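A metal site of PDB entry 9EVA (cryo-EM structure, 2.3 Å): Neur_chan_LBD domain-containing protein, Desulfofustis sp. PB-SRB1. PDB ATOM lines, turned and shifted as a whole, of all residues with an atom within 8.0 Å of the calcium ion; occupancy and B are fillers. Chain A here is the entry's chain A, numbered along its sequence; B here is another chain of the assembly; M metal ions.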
ATOM      1  N   MET A  68     -18.676  -5.321  -7.509  1.00  0.00           N
ATOM      2  CA  MET A  68     -19.111  -4.741  -8.771  1.00  0.00           C
ATOM      3  C   MET A  68     -17.898  -4.350  -9.592  1.00  0.00           C
ATOM      4  O   MET A  68     -17.045  -3.594  -9.112  1.00  0.00           O
ATOM      5  CB  MET A  68     -20.012  -3.518  -8.508  1.00  0.00           C
ATOM      6  CG  MET A  68     -20.708  -2.951  -9.727  1.00  0.00           C
ATOM      7  SD  MET A  68     -21.868  -1.659  -9.270  1.00  0.00           S
ATOM      8  CE  MET A  68     -22.335  -1.021 -10.874  1.00  0.00           C
ATOM      9  N   LEU A  75     -17.321   3.457 -16.629  1.00  0.00           N
ATOM     10  CA  LEU A  75     -18.110   3.374 -15.403  1.00  0.00           C
ATOM     11  C   LEU A  75     -17.223   3.230 -14.172  1.00  0.00           C
ATOM     12  O   LEU A  75     -16.245   2.491 -14.180  1.00  0.00           O
ATOM     13  CB  LEU A  75     -19.081   2.199 -15.497  1.00  0.00           C
ATOM     14  CG  LEU A  75     -19.927   1.900 -14.265  1.00  0.00           C
ATOM     15  CD1 LEU A  75     -20.811   3.091 -13.924  1.00  0.00           C
ATOM     16  CD2 LEU A  75     -20.768   0.661 -14.484  1.00  0.00           C
ATOM     17  N   ASP A  76     -17.580   3.953 -13.120  1.00  0.00           N
ATOM     18  CA  ASP A  76     -16.922   3.839 -11.816  1.00  0.00           C
ATOM     19  C   ASP A  76     -17.924   3.282 -10.804  1.00  0.00           C
ATOM     20  O   ASP A  76     -18.805   4.022 -10.345  1.00  0.00           O
ATOM     21  CB  ASP A  76     -16.400   5.191 -11.363  1.00  0.00           C
ATOM     22  CG  ASP A  76     -15.232   5.078 -10.406  1.00  0.00           C
ATOM     23  OD1 ASP A  76     -15.148   4.068  -9.681  1.00  0.00           O
ATOM     24  OD2 ASP A  76     -14.394   6.004 -10.384  1.00  0.00           O
ATOM     25  N   PRO A  77     -17.817   2.010 -10.433  1.00  0.00           N
ATOM     26  CA  PRO A  77     -18.874   1.369  -9.637  1.00  0.00           C
ATOM     27  C   PRO A  77     -19.044   1.975  -8.242  1.00  0.00           C
ATOM     28  O   PRO A  77     -18.095   2.471  -7.640  1.00  0.00           O
ATOM     29  CB  PRO A  77     -18.420  -0.085  -9.546  1.00  0.00           C
ATOM     30  CG  PRO A  77     -17.518  -0.279 -10.714  1.00  0.00           C
ATOM     31  CD  PRO A  77     -16.814   1.027 -10.886  1.00  0.00           C
ATOM     32  N   LEU A  78     -20.286   1.934  -7.754  1.00  0.00           N
ATOM     33  CA  LEU A  78     -20.636   2.275  -6.382  1.00  0.00           C
ATOM     34  C   LEU A  78     -21.791   1.386  -5.941  1.00  0.00           C
ATOM     35  O   LEU A  78     -22.711   1.122  -6.716  1.00  0.00           O
ATOM     36  CB  LEU A  78     -21.042   3.751  -6.271  1.00  0.00           C
ATOM     37  CG  LEU A  78     -21.630   4.199  -4.927  1.00  0.00           C
ATOM     38  CD1 LEU A  78     -20.623   4.019  -3.805  1.00  0.00           C
ATOM     39  CD2 LEU A  78     -22.088   5.651  -4.990  1.00  0.00           C
ATOM     40  N   VAL A  79     -21.736   0.913  -4.699  1.00  0.00           N
ATOM     41  CA  VAL A  79     -22.742   0.003  -4.161  1.00  0.00           C
ATOM     42  C   VAL A  79     -23.161   0.478  -2.770  1.00  0.00           C
ATOM     43  O   VAL A  79     -22.320   0.935  -1.985  1.00  0.00           O
ATOM     44  CB  VAL A  79     -22.231  -1.451  -4.119  1.00  0.00           C
ATOM     45  CG1 VAL A  79     -20.971  -1.570  -3.259  1.00  0.00           C
ATOM     46  CG2 VAL A  79     -23.317  -2.396  -3.632  1.00  0.00           C
ATOM     47  N   ASP A 122     -19.495   1.172  -0.303  1.00  0.00           N
ATOM     48  CA  ASP A 122     -18.077   1.075  -0.623  1.00  0.00           C
ATOM     49  C   ASP A 122     -17.859   1.638  -2.021  1.00  0.00           C
ATOM     50  O   ASP A 122     -18.669   1.406  -2.921  1.00  0.00           O
ATOM     51  CB  ASP A 122     -17.569  -0.362  -0.545  1.00  0.00           C
ATOM     52  CG  ASP A 122     -16.093  -0.480  -0.860  1.00  0.00           C
ATOM     53  OD1 ASP A 122     -15.271   0.018  -0.045  1.00  0.00           O
ATOM     54  OD2 ASP A 122     -15.739  -1.054  -1.904  1.00  0.00           O
ATOM     55  N   ASP A 123     -16.757   2.365  -2.192  1.00  0.00           N
ATOM     56  CA  ASP A 123     -16.434   2.983  -3.476  1.00  0.00           C
ATOM     57  C   ASP A 123     -15.339   2.224  -4.210  1.00  0.00           C
ATOM     58  O   ASP A 123     -15.562   1.755  -5.328  1.00  0.00           O
ATOM     59  CB  ASP A 123     -16.023   4.446  -3.255  1.00  0.00           C
ATOM     60  CG  ASP A 123     -16.144   5.285  -4.512  1.00  0.00           C
ATOM     61  OD1 ASP A 123     -16.065   4.714  -5.629  1.00  0.00           O
ATOM     62  OD2 ASP A 123     -16.317   6.507  -4.395  1.00  0.00           O
ATOM     63  N   ASP A 124     -14.151   2.073  -3.620  1.00  0.00           N
ATOM     64  CA  ASP A 124     -12.977   1.581  -4.323  1.00  0.00           C
ATOM     65  C   ASP A 124     -12.261   0.477  -3.544  1.00  0.00           C
ATOM     66  O   ASP A 124     -11.033   0.385  -3.552  1.00  0.00           O
ATOM     67  CB  ASP A 124     -12.004   2.722  -4.612  1.00  0.00           C
ATOM     68  CG  ASP A 124     -12.621   3.792  -5.489  1.00  0.00           C
ATOM     69  OD1 ASP A 124     -13.358   3.443  -6.434  1.00  0.00           O
ATOM     70  OD2 ASP A 124     -12.357   4.993  -5.229  1.00  0.00           O
ATOM     71  N   GLY A 125     -13.024  -0.381  -2.874  1.00  0.00           N
ATOM     72  CA  GLY A 125     -12.426  -1.400  -2.038  1.00  0.00           C
ATOM     73  C   GLY A 125     -11.807  -2.568  -2.763  1.00  0.00           C
ATOM     74  O   GLY A 125     -11.120  -3.381  -2.130  1.00  0.00           O
ATOM     75  N   GLY A 126     -12.036  -2.684  -4.075  1.00  0.00           N
ATOM     76  CA  GLY A 126     -11.558  -3.804  -4.843  1.00  0.00           C
ATOM     77  C   GLY A 126     -10.373  -3.453  -5.723  1.00  0.00           C
ATOM     78  O   GLY A 126      -9.680  -2.455  -5.520  1.00  0.00           O
ATOM     79  N   GLY A 128      -8.573  -1.871  -8.437  1.00  0.00           N
ATOM     80  CA  GLY A 128      -8.843  -0.679  -9.211  1.00  0.00           C
ATOM     81  C   GLY A 128      -9.948   0.144  -8.580  1.00  0.00           C
ATOM     82  O   GLY A 128      -9.920   0.422  -7.379  1.00  0.00           O
ATOM     83  N   TYR A 129     -10.928   0.542  -9.389  1.00  0.00           N
ATOM     84  CA  TYR A 129     -12.056   1.343  -8.921  1.00  0.00           C
ATOM     85  C   TYR A 129     -13.265   0.492  -8.576  1.00  0.00           C
ATOM     86  O   TYR A 129     -14.348   1.034  -8.322  1.00  0.00           O
ATOM     87  CB  TYR A 129     -12.421   2.385  -9.974  1.00  0.00           C
ATOM     88  CG  TYR A 129     -11.334   3.404 -10.239  1.00  0.00           C
ATOM     89  CD1 TYR A 129     -10.391   3.708  -9.277  1.00  0.00           C
ATOM     90  CD2 TYR A 129     -11.268   4.069 -11.453  1.00  0.00           C
ATOM     91  CE1 TYR A 129      -9.398   4.634  -9.521  1.00  0.00           C
ATOM     92  CE2 TYR A 129     -10.273   4.997 -11.711  1.00  0.00           C
ATOM     93  CZ  TYR A 129      -9.345   5.279 -10.732  1.00  0.00           C
ATOM     94  OH  TYR A 129      -8.362   6.200 -10.985  1.00  0.00           O
ATOM     95  N   SER A 130     -13.112  -0.824  -8.540  1.00  0.00           N
ATOM     96  CA  SER A 130     -14.220  -1.723  -8.244  1.00  0.00           C
ATOM     97  C   SER A 130     -14.533  -1.708  -6.750  1.00  0.00           C
ATOM     98  O   SER A 130     -13.656  -1.490  -5.914  1.00  0.00           O
ATOM     99  CB  SER A 130     -13.887  -3.144  -8.697  1.00  0.00           C
ATOM    100  OG  SER A 130     -12.728  -3.630  -8.031  1.00  0.00           O
ATOM    101  N   ALA A 131     -15.799  -1.950  -6.423  1.00  0.00           N
ATOM    102  CA  ALA A 131     -16.287  -1.902  -5.049  1.00  0.00           C
ATOM    103  C   ALA A 131     -16.453  -3.304  -4.477  1.00  0.00           C
ATOM    104  O   ALA A 131     -16.691  -4.267  -5.211  1.00  0.00           O
ATOM    105  CB  ALA A 131     -17.618  -1.163  -4.973  1.00  0.00           C
ATOM    106  N   SER A 132     -16.313  -3.409  -3.156  1.00  0.00           N
ATOM    107  CA  SER A 132     -16.540  -4.651  -2.433  1.00  0.00           C
ATOM    108  C   SER A 132     -17.064  -4.307  -1.055  1.00  0.00           C
ATOM    109  O   SER A 132     -16.531  -3.410  -0.389  1.00  0.00           O
ATOM    110  CB  SER A 132     -15.260  -5.477  -2.338  1.00  0.00           C
ATOM    111  OG  SER A 132     -14.210  -4.740  -1.747  1.00  0.00           O
ATOM    112  N   GLY A 148     -24.834   1.674  -8.976  1.00  0.00           N
ATOM    113  CA  GLY A 148     -24.825   2.883  -9.768  1.00  0.00           C
ATOM    114  C   GLY A 148     -23.437   3.440  -9.961  1.00  0.00           C
ATOM    115  O   GLY A 148     -22.447   2.705  -9.896  1.00  0.00           O
ATOM    116  N   SER A 149     -23.372   4.750 -10.205  1.00  0.00           N
ATOM    117  CA  SER A 149     -22.136   5.443 -10.512  1.00  0.00           C
ATOM    118  C   SER A 149     -21.837   6.490  -9.446  1.00  0.00           C
ATOM    119  O   SER A 149     -22.741   7.198  -9.000  1.00  0.00           O
ATOM    120  CB  SER A 149     -22.222   6.115 -11.889  1.00  0.00           C
ATOM    121  OG  SER A 149     -21.081   6.906 -12.148  1.00  0.00           O
ATOM    122  N   THR A 150     -20.570   6.566  -9.037  1.00  0.00           N
ATOM    123  CA  THR A 150     -20.140   7.617  -8.125  1.00  0.00           C
ATOM    124  C   THR A 150     -19.811   8.898  -8.903  1.00  0.00           C
ATOM    125  O   THR A 150     -19.897   8.950 -10.128  1.00  0.00           O
ATOM    126  CB  THR A 150     -18.923   7.160  -7.327  1.00  0.00           C
ATOM    127  OG1 THR A 150     -18.424   8.245  -6.531  1.00  0.00           O
ATOM    128  CG2 THR A 150     -17.821   6.681  -8.260  1.00  0.00           C
ATOM    129  N   ILE A 151     -19.434   9.930  -8.157  1.00  0.00           N
ATOM    130  CA  ILE A 151     -19.037  11.216  -8.732  1.00  0.00           C
ATOM    131  C   ILE A 151     -17.519  11.297  -8.705  1.00  0.00           C
ATOM    132  O   ILE A 151     -16.905  11.250  -7.637  1.00  0.00           O
ATOM    133  CB  ILE A 151     -19.672  12.381  -7.966  1.00  0.00           C
ATOM    134  CG1 ILE A 151     -21.191  12.280  -8.002  1.00  0.00           C
ATOM    135  CG2 ILE A 151     -19.201  13.708  -8.533  1.00  0.00           C
ATOM    136  CD1 ILE A 151     -21.886  13.378  -7.223  1.00  0.00           C
ATOM    137  N   THR A 152     -16.911  11.442  -9.885  1.00  0.00           N
ATOM    138  CA  THR A 152     -15.460  11.405 -10.008  1.00  0.00           C
ATOM    139  C   THR A 152     -14.998  12.429 -11.038  1.00  0.00           C
ATOM    140  O   THR A 152     -15.792  12.974 -11.807  1.00  0.00           O
ATOM    141  CB  THR A 152     -14.955  10.012 -10.428  1.00  0.00           C
ATOM    142  OG1 THR A 152     -15.617   9.607 -11.635  1.00  0.00           O
ATOM    143  CG2 THR A 152     -15.231   8.991  -9.344  1.00  0.00           C
ATOM    144  N   LYS B 255      -8.606  10.662 -10.114  1.00  0.00           N
ATOM    145  CA  LYS B 255      -9.426  10.451  -8.926  1.00  0.00           C
ATOM    146  C   LYS B 255      -8.922  11.339  -7.791  1.00  0.00           C
ATOM    147  O   LYS B 255      -7.745  11.281  -7.431  1.00  0.00           O
ATOM    148  CB  LYS B 255      -9.369   8.986  -8.503  1.00  0.00           C
ATOM    149  CG  LYS B 255     -10.685   8.252  -8.577  1.00  0.00           C
ATOM    150  CD  LYS B 255     -11.488   8.438  -7.310  1.00  0.00           C
ATOM    151  CE  LYS B 255     -12.720   7.551  -7.310  1.00  0.00           C
ATOM    152  NZ  LYS B 255     -12.378   6.138  -7.588  1.00  0.00           N
HETATM  153 CA    CA M   1     -15.533   3.078  -7.418  1.00  0.00          CA
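Five residues have an atom within 4 Å of the calcium ion: Asp 76, Pro 77, Asp 123, Asp 124 and Tyr 129.
The nearest printed residue that does not touch the calcium ion is Thr 150 (4.4 Å).
OD1 of Asp 124 binds the calcium ion (2.4 Å).
The backbone carbonyl oxygen (O) of Asp 123 binds the calcium ion (2.5 Å).
The calcium ion is bound by the side-chain carboxylate (OD1) of Asp 123 (2.5 Å).
The side-chain carboxylate (OD1) of Asp 76 binds the calcium ion.
O of Tyr 129 is bound to the calcium ion (2.5 Å).
The calcium ion is bound by O of Pro 77 (2.6 Å).
The calcium ion has six donor atoms within binding distance.
OD2 of Asp 123 is in hydrogen-bond range of OG1 of Thr 150 (3.5 Å).
The side-chain amino group of Lys 255 of chain B is in salt-bridge range of the side-chain carboxylate of Asp 124 (2.6 Å).
O of Asp 76 lies within hydrogen-bond range of N of Thr 150 (3.4 Å).
The side-chain carboxylate (OD2) of Asp 76 lies within salt-bridge range of the side-chain amino group (NZ) of Lys 255 of chain B, 3.4 Å away.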
